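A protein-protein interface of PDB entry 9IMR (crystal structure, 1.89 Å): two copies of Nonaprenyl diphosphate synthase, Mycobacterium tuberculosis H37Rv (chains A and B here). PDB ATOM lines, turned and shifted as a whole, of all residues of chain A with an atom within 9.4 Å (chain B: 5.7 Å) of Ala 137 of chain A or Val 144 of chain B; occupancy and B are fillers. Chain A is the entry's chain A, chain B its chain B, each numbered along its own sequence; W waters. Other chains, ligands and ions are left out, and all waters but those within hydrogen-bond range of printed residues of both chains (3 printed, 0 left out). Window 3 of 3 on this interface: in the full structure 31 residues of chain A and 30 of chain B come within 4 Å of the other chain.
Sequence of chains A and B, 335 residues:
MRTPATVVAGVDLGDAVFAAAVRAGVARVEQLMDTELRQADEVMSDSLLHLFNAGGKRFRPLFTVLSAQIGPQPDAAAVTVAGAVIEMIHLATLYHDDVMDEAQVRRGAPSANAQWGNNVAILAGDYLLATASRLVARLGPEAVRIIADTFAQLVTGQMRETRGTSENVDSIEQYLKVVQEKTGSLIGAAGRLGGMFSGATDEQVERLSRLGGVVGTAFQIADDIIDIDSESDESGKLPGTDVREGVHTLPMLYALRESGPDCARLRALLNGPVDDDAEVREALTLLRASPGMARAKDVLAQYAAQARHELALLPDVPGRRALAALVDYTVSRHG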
ATOM      1  N   VAL A  81      -4.028  29.320  -8.495  1.00  0.00           N
ATOM      2  CA  VAL A  81      -3.837  28.686  -7.169  1.00  0.00           C
ATOM      3  C   VAL A  81      -3.364  27.241  -7.387  1.00  0.00           C
ATOM      4  O   VAL A  81      -2.415  26.824  -6.731  1.00  0.00           O
ATOM      5  CB  VAL A  81      -5.130  28.757  -6.329  1.00  0.00           C
ATOM      6  CG1 VAL A  81      -4.972  27.967  -5.040  1.00  0.00           C
ATOM      7  CG2 VAL A  81      -5.523  30.206  -6.013  1.00  0.00           C
ATOM      8  N   ALA A  82      -4.052  26.481  -8.248  1.00  0.00           N
ATOM      9  CA  ALA A  82      -3.707  25.074  -8.536  1.00  0.00           C
ATOM     10  C   ALA A  82      -2.260  24.978  -9.022  1.00  0.00           C
ATOM     11  O   ALA A  82      -1.522  24.096  -8.534  1.00  0.00           O
ATOM     12  CB  ALA A  82      -4.681  24.505  -9.535  1.00  0.00           C
ATOM     13  N   VAL A  85       0.066  25.499  -6.132  1.00  0.00           N
ATOM     14  CA  VAL A  85       0.046  24.348  -5.208  1.00  0.00           C
ATOM     15  C   VAL A  85       0.945  23.235  -5.782  1.00  0.00           C
ATOM     16  O   VAL A  85       1.732  22.667  -5.033  1.00  0.00           O
ATOM     17  CB  VAL A  85      -1.388  23.850  -4.980  1.00  0.00           C
ATOM     18  CG1 VAL A  85      -1.382  22.491  -4.288  1.00  0.00           C
ATOM     19  CG2 VAL A  85      -2.179  24.881  -4.183  1.00  0.00           C
ATOM     20  N   LEU A 129       5.325  21.999   2.374  1.00  0.00           N
ATOM     21  CA  LEU A 129       4.135  21.137   2.446  1.00  0.00           C
ATOM     22  C   LEU A 129       3.041  21.881   3.176  1.00  0.00           C
ATOM     23  O   LEU A 129       1.907  21.818   2.717  1.00  0.00           O
ATOM     24  CB  LEU A 129       4.452  19.822   3.158  1.00  0.00           C
ATOM     25  CG  LEU A 129       5.421  18.899   2.434  1.00  0.00           C
ATOM     26  CD1 LEU A 129       5.512  17.594   3.235  1.00  0.00           C
ATOM     27  CD2 LEU A 129       4.962  18.639   0.993  1.00  0.00           C
ATOM     28  N   ALA A 130       3.367  22.599   4.254  1.00  0.00           N
ATOM     29  CA  ALA A 130       2.377  23.376   5.028  1.00  0.00           C
ATOM     30  C   ALA A 130       1.835  24.497   4.149  1.00  0.00           C
ATOM     31  O   ALA A 130       0.618  24.763   4.189  1.00  0.00           O
ATOM     32  CB  ALA A 130       3.000  23.926   6.293  1.00  0.00           C
ATOM     33  N   THR A 131       2.720  25.143   3.396  1.00  0.00           N
ATOM     34  CA  THR A 131       2.369  26.245   2.467  1.00  0.00           C
ATOM     35  C   THR A 131       1.390  25.704   1.416  1.00  0.00           C
ATOM     36  O   THR A 131       0.350  26.349   1.160  1.00  0.00           O
ATOM     37  CB  THR A 131       3.627  26.851   1.853  1.00  0.00           C
ATOM     38  OG1 THR A 131       4.431  27.325   2.934  1.00  0.00           O
ATOM     39  CG2 THR A 131       3.326  27.997   0.918  1.00  0.00           C
ATOM     40  N   ALA A 132       1.758  24.611   0.766  1.00  0.00           N
ATOM     41  CA  ALA A 132       0.943  23.976  -0.292  1.00  0.00           C
ATOM     42  C   ALA A 132      -0.435  23.623   0.274  1.00  0.00           C
ATOM     43  O   ALA A 132      -1.502  23.859  -0.389  1.00  0.00           O
ATOM     44  CB  ALA A 132       1.657  22.762  -0.811  1.00  0.00           C
ATOM     45  N   SER A 133      -0.418  23.044   1.468  1.00  0.00           N
ATOM     46  CA  SER A 133      -1.629  22.640   2.200  1.00  0.00           C
ATOM     47  C   SER A 133      -2.513  23.863   2.411  1.00  0.00           C
ATOM     48  O   SER A 133      -3.723  23.787   2.124  1.00  0.00           O
ATOM     49  CB  SER A 133      -1.248  21.973   3.498  1.00  0.00           C
ATOM     50  OG  SER A 133      -2.405  21.614   4.213  1.00  0.00           O
ATOM     51  N   ARG A 134      -1.955  24.978   2.879  1.00  0.00           N
ATOM     52  CA  ARG A 134      -2.805  26.144   3.214  1.00  0.00           C
ATOM     53  C   ARG A 134      -3.354  26.749   1.917  1.00  0.00           C
ATOM     54  O   ARG A 134      -4.499  27.148   1.901  1.00  0.00           O
ATOM     55  CB  ARG A 134      -2.036  27.160   4.053  1.00  0.00           C
ATOM     56  CG  ARG A 134      -2.929  28.287   4.561  1.00  0.00           C
ATOM     57  CD  ARG A 134      -2.290  29.030   5.717  1.00  0.00           C
ATOM     58  NE  ARG A 134      -0.837  29.071   5.549  1.00  0.00           N
ATOM     59  CZ  ARG A 134      -0.173  29.864   4.696  1.00  0.00           C
ATOM     60  NH1 ARG A 134      -0.820  30.717   3.916  1.00  0.00           N
ATOM     61  NH2 ARG A 134       1.148  29.794   4.626  1.00  0.00           N
ATOM     62  N   LEU A 135      -2.566  26.776   0.856  1.00  0.00           N
ATOM     63  CA  LEU A 135      -2.980  27.285  -0.479  1.00  0.00           C
ATOM     64  C   LEU A 135      -4.097  26.416  -1.071  1.00  0.00           C
ATOM     65  O   LEU A 135      -5.093  26.973  -1.560  1.00  0.00           O
ATOM     66  CB  LEU A 135      -1.728  27.292  -1.357  1.00  0.00           C
ATOM     67  CG  LEU A 135      -1.671  28.264  -2.520  1.00  0.00           C
ATOM     68  CD1 LEU A 135      -2.229  29.640  -2.151  1.00  0.00           C
ATOM     69  CD2 LEU A 135      -0.235  28.379  -2.998  1.00  0.00           C
ATOM     70  N   VAL A 136      -3.935  25.105  -1.091  1.00  0.00           N
ATOM     71  CA  VAL A 136      -4.919  24.217  -1.767  1.00  0.00           C
ATOM     72  C   VAL A 136      -6.245  24.268  -1.001  1.00  0.00           C
ATOM     73  O   VAL A 136      -7.257  24.067  -1.670  1.00  0.00           O
ATOM     74  CB  VAL A 136      -4.447  22.774  -1.968  1.00  0.00           C
ATOM     75  CG1 VAL A 136      -4.401  22.001  -0.685  1.00  0.00           C
ATOM     76  CG2 VAL A 136      -5.341  22.063  -2.962  1.00  0.00           C
ATOM     77  N   ALA A 137      -6.234  24.624   0.293  1.00  0.00           N
ATOM     78  CA  ALA A 137      -7.460  24.777   1.114  1.00  0.00           C
ATOM     79  C   ALA A 137      -8.396  25.792   0.443  1.00  0.00           C
ATOM     80  O   ALA A 137      -9.627  25.569   0.441  1.00  0.00           O
ATOM     81  CB  ALA A 137      -7.118  25.152   2.552  1.00  0.00           C
ATOM     82  N   ARG A 138      -7.836  26.783  -0.249  1.00  0.00           N
ATOM     83  CA  ARG A 138      -8.627  27.780  -1.013  1.00  0.00           C
ATOM     84  C   ARG A 138      -9.519  27.107  -2.061  1.00  0.00           C
ATOM     85  O   ARG A 138     -10.488  27.736  -2.449  1.00  0.00           O
ATOM     86  CB  ARG A 138      -7.746  28.768  -1.772  1.00  0.00           C
ATOM     87  CG  ARG A 138      -6.956  29.703  -0.879  1.00  0.00           C
ATOM     88  CD  ARG A 138      -6.379  30.836  -1.699  1.00  0.00           C
ATOM     89  NE  ARG A 138      -5.232  31.360  -0.999  1.00  0.00           N
ATOM     90  CZ  ARG A 138      -4.439  32.314  -1.469  1.00  0.00           C
ATOM     91  NH1 ARG A 138      -3.409  32.715  -0.745  1.00  0.00           N
ATOM     92  NH2 ARG A 138      -4.668  32.836  -2.662  1.00  0.00           N
ATOM     93  N   LEU A 139      -9.171  25.919  -2.564  1.00  0.00           N
ATOM     94  CA  LEU A 139      -9.822  25.344  -3.771  1.00  0.00           C
ATOM     95  C   LEU A 139     -10.944  24.408  -3.350  1.00  0.00           C
ATOM     96  O   LEU A 139     -11.666  23.909  -4.210  1.00  0.00           O
ATOM     97  CB  LEU A 139      -8.775  24.590  -4.587  1.00  0.00           C
ATOM     98  CG  LEU A 139      -7.701  25.457  -5.245  1.00  0.00           C
ATOM     99  CD1 LEU A 139      -6.747  24.611  -6.070  1.00  0.00           C
ATOM    100  CD2 LEU A 139      -8.306  26.527  -6.109  1.00  0.00           C
ATOM    101  N   GLY A 140     -10.997  24.078  -2.067  1.00  0.00           N
ATOM    102  CA  GLY A 140     -12.085  23.270  -1.502  1.00  0.00           C
ATOM    103  C   GLY A 140     -11.665  21.837  -1.227  1.00  0.00           C
ATOM    104  O   GLY A 140     -10.556  21.427  -1.532  1.00  0.00           O
ATOM    105  N   PRO A 141     -12.561  21.043  -0.618  1.00  0.00           N
ATOM    106  CA  PRO A 141     -12.184  19.730  -0.088  1.00  0.00           C
ATOM    107  C   PRO A 141     -11.783  18.716  -1.161  1.00  0.00           C
ATOM    108  O   PRO A 141     -10.912  17.893  -0.894  1.00  0.00           O
ATOM    109  CB  PRO A 141     -13.424  19.262   0.694  1.00  0.00           C
ATOM    110  CG  PRO A 141     -14.564  20.136   0.186  1.00  0.00           C
ATOM    111  CD  PRO A 141     -13.933  21.442  -0.258  1.00  0.00           C
ATOM    112  N   GLU A 142     -12.376  18.785  -2.352  1.00  0.00           N
ATOM    113  CA  GLU A 142     -11.996  17.848  -3.452  1.00  0.00           C
ATOM    114  C   GLU A 142     -10.506  18.037  -3.777  1.00  0.00           C
ATOM    115  O   GLU A 142      -9.772  17.007  -3.941  1.00  0.00           O
ATOM    116  CB  GLU A 142     -12.819  18.097  -4.712  1.00  0.00           C
ATOM    117  CG  GLU A 142     -13.817  17.027  -5.062  1.00  0.00           C
ATOM    118  CD  GLU A 142     -13.859  16.760  -6.563  1.00  0.00           C
ATOM    119  OE1 GLU A 142     -13.307  15.712  -7.006  1.00  0.00           O
ATOM    120  OE2 GLU A 142     -14.420  17.613  -7.295  1.00  0.00           O
ATOM    121  N   ALA A 143     -10.082  19.282  -3.948  1.00  0.00           N
ATOM    122  CA  ALA A 143      -8.675  19.628  -4.286  1.00  0.00           C
ATOM    123  C   ALA A 143      -7.749  19.229  -3.133  1.00  0.00           C
ATOM    124  O   ALA A 143      -6.658  18.695  -3.354  1.00  0.00           O
ATOM    125  CB  ALA A 143      -8.619  21.094  -4.565  1.00  0.00           C
ATOM    126  N   VAL A 144      -8.176  19.467  -1.898  1.00  0.00           N
ATOM    127  CA  VAL A 144      -7.383  19.106  -0.702  1.00  0.00           C
ATOM    128  C   VAL A 144      -7.067  17.611  -0.744  1.00  0.00           C
ATOM    129  O   VAL A 144      -5.871  17.245  -0.518  1.00  0.00           O
ATOM    130  CB  VAL A 144      -8.085  19.497   0.608  1.00  0.00           C
ATOM    131  CG1 VAL A 144      -7.349  18.922   1.803  1.00  0.00           C
ATOM    132  CG2 VAL A 144      -8.140  21.013   0.736  1.00  0.00           C
ATOM    133  N   ARG A 145      -8.092  16.795  -0.969  1.00  0.00           N
ATOM    134  CA  ARG A 145      -7.968  15.320  -1.043  1.00  0.00           C
ATOM    135  C   ARG A 145      -7.033  14.944  -2.197  1.00  0.00           C
ATOM    136  O   ARG A 145      -6.200  14.042  -2.011  1.00  0.00           O
ATOM    137  CB  ARG A 145      -9.346  14.678  -1.221  1.00  0.00           C
ATOM    138  CG  ARG A 145      -9.304  13.185  -1.511  1.00  0.00           C
ATOM    139  CD  ARG A 145      -8.613  12.454  -0.371  1.00  0.00           C
ATOM    140  NE  ARG A 145      -9.040  11.056  -0.256  1.00  0.00           N
ATOM    141  CZ  ARG A 145      -9.786  10.562   0.733  1.00  0.00           C
ATOM    142  NH1 ARG A 145     -10.176  11.337   1.735  1.00  0.00           N
ATOM    143  NH2 ARG A 145     -10.115   9.277   0.732  1.00  0.00           N
ATOM    144  N   ILE A 147      -4.583  16.549  -3.597  1.00  0.00           N
ATOM    145  CA  ILE A 147      -3.184  16.931  -3.275  1.00  0.00           C
ATOM    146  C   ILE A 147      -2.628  15.983  -2.187  1.00  0.00           C
ATOM    147  O   ILE A 147      -1.477  15.524  -2.367  1.00  0.00           O
ATOM    148  CB  ILE A 147      -3.077  18.428  -2.955  1.00  0.00           C
ATOM    149  CG1 ILE A 147      -3.220  19.271  -4.228  1.00  0.00           C
ATOM    150  CG2 ILE A 147      -1.781  18.749  -2.237  1.00  0.00           C
ATOM    151  CD1 ILE A 147      -2.300  18.851  -5.390  1.00  0.00           C
ATOM    152  N   ALA A 148      -3.415  15.639  -1.149  1.00  0.00           N
ATOM    153  CA  ALA A 148      -3.025  14.677  -0.097  1.00  0.00           C
ATOM    154  C   ALA A 148      -2.695  13.330  -0.739  1.00  0.00           C
ATOM    155  O   ALA A 148      -1.635  12.771  -0.436  1.00  0.00           O
ATOM    156  CB  ALA A 148      -4.114  14.530   0.943  1.00  0.00           C
ATOM    157  N   PHE A 197     -10.507  23.353 -12.566  1.00  0.00           N
ATOM    158  CA  PHE A 197     -10.736  24.757 -12.145  1.00  0.00           C
ATOM    159  C   PHE A 197     -10.902  25.673 -13.349  1.00  0.00           C
ATOM    160  O   PHE A 197     -11.229  26.849 -13.169  1.00  0.00           O
ATOM    161  CB  PHE A 197      -9.688  25.148 -11.111  1.00  0.00           C
ATOM    162  CG  PHE A 197     -10.004  24.425  -9.833  1.00  0.00           C
ATOM    163  CD1 PHE A 197     -11.051  24.845  -9.030  1.00  0.00           C
ATOM    164  CD2 PHE A 197      -9.240  23.360  -9.411  1.00  0.00           C
ATOM    165  CE1 PHE A 197     -11.393  24.145  -7.884  1.00  0.00           C
ATOM    166  CE2 PHE A 197      -9.543  22.695  -8.240  1.00  0.00           C
ATOM    167  CZ  PHE A 197     -10.633  23.083  -7.476  1.00  0.00           C
ATOM    168  N   SER B 133      -3.024  15.110   6.484  1.00  0.00           N
ATOM    169  CA  SER B 133      -3.692  16.043   5.551  1.00  0.00           C
ATOM    170  C   SER B 133      -5.024  15.457   5.048  1.00  0.00           C
ATOM    171  O   SER B 133      -6.001  16.174   5.053  1.00  0.00           O
ATOM    172  CB  SER B 133      -2.774  16.408   4.397  1.00  0.00           C
ATOM    173  OG  SER B 133      -3.438  17.306   3.538  1.00  0.00           O
ATOM    174  N   VAL B 136      -7.507  15.205   8.276  1.00  0.00           N
ATOM    175  CA  VAL B 136      -8.026  16.500   8.809  1.00  0.00           C
ATOM    176  C   VAL B 136      -9.060  17.056   7.827  1.00  0.00           C
ATOM    177  O   VAL B 136      -9.970  17.768   8.268  1.00  0.00           O
ATOM    178  CB  VAL B 136      -6.897  17.509   9.086  1.00  0.00           C
ATOM    179  CG1 VAL B 136      -6.297  18.100   7.818  1.00  0.00           C
ATOM    180  CG2 VAL B 136      -7.397  18.623   9.998  1.00  0.00           C
ATOM    181  N   ALA B 137      -8.943  16.740   6.536  1.00  0.00           N
ATOM    182  CA  ALA B 137      -9.926  17.138   5.504  1.00  0.00           C
ATOM    183  C   ALA B 137     -11.337  16.723   5.964  1.00  0.00           C
ATOM    184  O   ALA B 137     -12.264  17.517   5.786  1.00  0.00           O
ATOM    185  CB  ALA B 137      -9.548  16.536   4.169  1.00  0.00           C
ATOM    186  N   GLY B 140     -13.334  19.476   8.022  1.00  0.00           N
ATOM    187  CA  GLY B 140     -13.790  20.744   7.436  1.00  0.00           C
ATOM    188  C   GLY B 140     -12.669  21.768   7.297  1.00  0.00           C
ATOM    189  O   GLY B 140     -11.560  21.604   7.817  1.00  0.00           O
ATOM    190  N   PRO B 141     -12.938  22.849   6.547  1.00  0.00           N
ATOM    191  CA  PRO B 141     -11.906  23.808   6.159  1.00  0.00           C
ATOM    192  C   PRO B 141     -11.245  24.564   7.312  1.00  0.00           C
ATOM    193  O   PRO B 141     -10.079  24.893   7.183  1.00  0.00           O
ATOM    194  CB  PRO B 141     -12.597  24.849   5.247  1.00  0.00           C
ATOM    195  CG  PRO B 141     -14.086  24.523   5.328  1.00  0.00           C
ATOM    196  CD  PRO B 141     -14.240  23.136   5.928  1.00  0.00           C
ATOM    197  N   GLU B 142     -11.984  24.873   8.379  1.00  0.00           N
ATOM    198  CA  GLU B 142     -11.388  25.590   9.530  1.00  0.00           C
ATOM    199  C   GLU B 142     -10.283  24.695  10.127  1.00  0.00           C
ATOM    200  O   GLU B 142      -9.171  25.209  10.344  1.00  0.00           O
ATOM    201  CB  GLU B 142     -12.444  26.022  10.552  1.00  0.00           C
ATOM    202  CG  GLU B 142     -11.842  26.752  11.735  1.00  0.00           C
ATOM    203  CD  GLU B 142     -12.624  27.909  12.361  1.00  0.00           C
ATOM    204  OE1 GLU B 142     -13.858  27.777  12.577  1.00  0.00           O
ATOM    205  OE2 GLU B 142     -11.976  28.941  12.668  1.00  0.00           O
ATOM    206  N   ALA B 143     -10.563  23.414  10.369  1.00  0.00           N
ATOM    207  CA  ALA B 143      -9.575  22.467  10.927  1.00  0.00           C
ATOM    208  C   ALA B 143      -8.397  22.309   9.959  1.00  0.00           C
ATOM    209  O   ALA B 143      -7.259  22.203  10.437  1.00  0.00           O
ATOM    210  CB  ALA B 143     -10.205  21.146  11.223  1.00  0.00           C
ATOM    211  N   VAL B 144      -8.648  22.243   8.646  1.00  0.00           N
ATOM    212  CA  VAL B 144      -7.554  22.155   7.626  1.00  0.00           C
ATOM    213  C   VAL B 144      -6.603  23.324   7.809  1.00  0.00           C
ATOM    214  O   VAL B 144      -5.382  23.099   7.820  1.00  0.00           O
ATOM    215  CB  VAL B 144      -8.107  22.119   6.194  1.00  0.00           C
ATOM    216  CG1 VAL B 144      -7.019  22.419   5.162  1.00  0.00           C
ATOM    217  CG2 VAL B 144      -8.779  20.787   5.946  1.00  0.00           C
ATOM    218  N   ARG B 145      -7.143  24.543   7.909  1.00  0.00           N
ATOM    219  CA  ARG B 145      -6.341  25.786   8.044  1.00  0.00           C
ATOM    220  C   ARG B 145      -5.585  25.752   9.380  1.00  0.00           C
ATOM    221  O   ARG B 145      -4.409  26.090   9.385  1.00  0.00           O
ATOM    222  CB  ARG B 145      -7.217  27.042   7.958  1.00  0.00           C
ATOM    223  CG  ARG B 145      -7.433  27.546   6.530  1.00  0.00           C
ATOM    224  CD  ARG B 145      -8.804  28.143   6.197  1.00  0.00           C
ATOM    225  NE  ARG B 145      -9.429  28.806   7.342  1.00  0.00           N
ATOM    226  CZ  ARG B 145     -10.725  28.758   7.675  1.00  0.00           C
ATOM    227  NH1 ARG B 145     -11.597  28.075   6.944  1.00  0.00           N
ATOM    228  NH2 ARG B 145     -11.136  29.402   8.762  1.00  0.00           N
ATOM    229  N   ILE B 146      -6.241  25.352  10.466  1.00  0.00           N
ATOM    230  CA  ILE B 146      -5.587  25.288  11.799  1.00  0.00           C
ATOM    231  C   ILE B 146      -4.370  24.360  11.686  1.00  0.00           C
ATOM    232  O   ILE B 146      -3.285  24.744  12.156  1.00  0.00           O
ATOM    233  CB  ILE B 146      -6.580  24.808  12.859  1.00  0.00           C
ATOM    234  CG1 ILE B 146      -7.644  25.871  13.147  1.00  0.00           C
ATOM    235  CG2 ILE B 146      -5.877  24.384  14.137  1.00  0.00           C
ATOM    236  CD1 ILE B 146      -8.891  25.268  13.750  1.00  0.00           C
ATOM    237  N   ILE B 147      -4.528  23.191  11.065  1.00  0.00           N
ATOM    238  CA  ILE B 147      -3.446  22.169  11.049  1.00  0.00           C
ATOM    239  C   ILE B 147      -2.302  22.645  10.133  1.00  0.00           C
ATOM    240  O   ILE B 147      -1.132  22.500  10.525  1.00  0.00           O
ATOM    241  CB  ILE B 147      -4.028  20.792  10.696  1.00  0.00           C
ATOM    242  CG1 ILE B 147      -4.748  20.195  11.898  1.00  0.00           C
ATOM    243  CG2 ILE B 147      -2.967  19.848  10.190  1.00  0.00           C
ATOM    244  CD1 ILE B 147      -3.900  20.045  13.140  1.00  0.00           C
ATOM    245  N   ALA B 148      -2.616  23.247   8.976  1.00  0.00           N
ATOM    246  CA  ALA B 148      -1.574  23.801   8.089  1.00  0.00           C
ATOM    247  C   ALA B 148      -0.793  24.882   8.836  1.00  0.00           C
ATOM    248  O   ALA B 148       0.445  24.891   8.764  1.00  0.00           O
ATOM    249  CB  ALA B 148      -2.146  24.320   6.801  1.00  0.00           C
ATOM    250  N   ASP B 149      -1.477  25.760   9.541  1.00  0.00           N
ATOM    251  CA  ASP B 149      -0.818  26.888  10.240  1.00  0.00           C
ATOM    252  C   ASP B 149       0.047  26.316  11.370  1.00  0.00           C
ATOM    253  O   ASP B 149       1.176  26.840  11.598  1.00  0.00           O
ATOM    254  CB  ASP B 149      -1.831  27.918  10.750  1.00  0.00           C
ATOM    255  CG  ASP B 149      -2.356  28.859   9.672  1.00  0.00           C
ATOM    256  OD1 ASP B 149      -1.722  28.966   8.597  1.00  0.00           O
ATOM    257  OD2 ASP B 149      -3.423  29.438   9.912  1.00  0.00           O
HETATM  258  O   HOH W   1      -3.841  18.620   0.745  1.00  0.00           O
HETATM  259  O   HOH W   2      -4.455  20.449   2.636  1.00  0.00           O
HETATM  260  O   HOH W   3      -4.144  20.761   6.852  1.00  0.00           O
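Ala 82 of chain A touches none of the printed residues of chain B.
Printed residues of chain B within 4 Å of Ser 133 of chain A: Ala 148 (3.8 Å).
Printed residues of chain B within 4 Å of Arg 134 of chain A: Ala 148 and Asp 149.
Ala 137 of chain A touches one residue of chain B.
Gly 140 of chain B touches none of the printed residues of chain A.
Of chain A, only Ala 137 comes within 4 Å of Val 144 of chain B.
Of the printed residues of chain A, Ala 148 of chain B touches Ala 130 (3.7 Å), Ser 133 (3.8 Å) and Arg 134 (3.95 Å).
Of the printed residues of chain A, Asp 149 of chain B touches Arg 134.
The nearest residue of chain B that does not touch Ala 137 of chain A is Arg 145 of chain B (4.7 Å).
The nearest printed residue of chain A that does not touch Ala 148 of chain B is Thr 131 of chain A (5.8 Å).
Ser 133 of chain A touches Ala 148 of chain B, and with the chains exchanged Ala 148 of chain A touches Ser 133 of chain B.
Ala 137 of chain A touches Val 144 of chain B, but with the chains exchanged Val 144 of chain A does not touch Ala 137 of chain B (4.02 Å).
11 positions are printed for both chains.
Water W1 bridges the backbone carbonyl oxygen of Val 144 of chain A (2.8 Å) and the side-chain hydroxyl of Ser 133 of chain B (3.1 Å).
Water W3 bridges O of Val 144 of chain B (2.8 Å) and OG of Ser 133 of chain A (3.3 Å).
Water W2 lies within hydrogen-bond range of the side-chain hydroxyl (OG) of Ser 133 of chain A and the side-chain hydroxyl (OG) of Ser 133 of chain B.
Of the 13 printed residues of chain B, 4 touch a printed residue of chain A.
The side-chain carboxylate (OD1) of Asp 149 of chain B lies within salt-bridge range of the guanidinium group (NE) of Arg 134 of chain A (3.2 Å).
Among the printed residues, merely in contact across the chains: Ala 130 of chain A with Ala 148 of chain B (3.7 Å), Ser 133 of chain A with Ala 148 of chain B (3.8 Å), Arg 134 of chain A with Ala 148 of chain B (3.95 Å), Ala 137 of chain A with Val 144 of chain B (3.8 Å) and Ala 148 of chain A with Ser 133 of chain B (3.9 Å).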
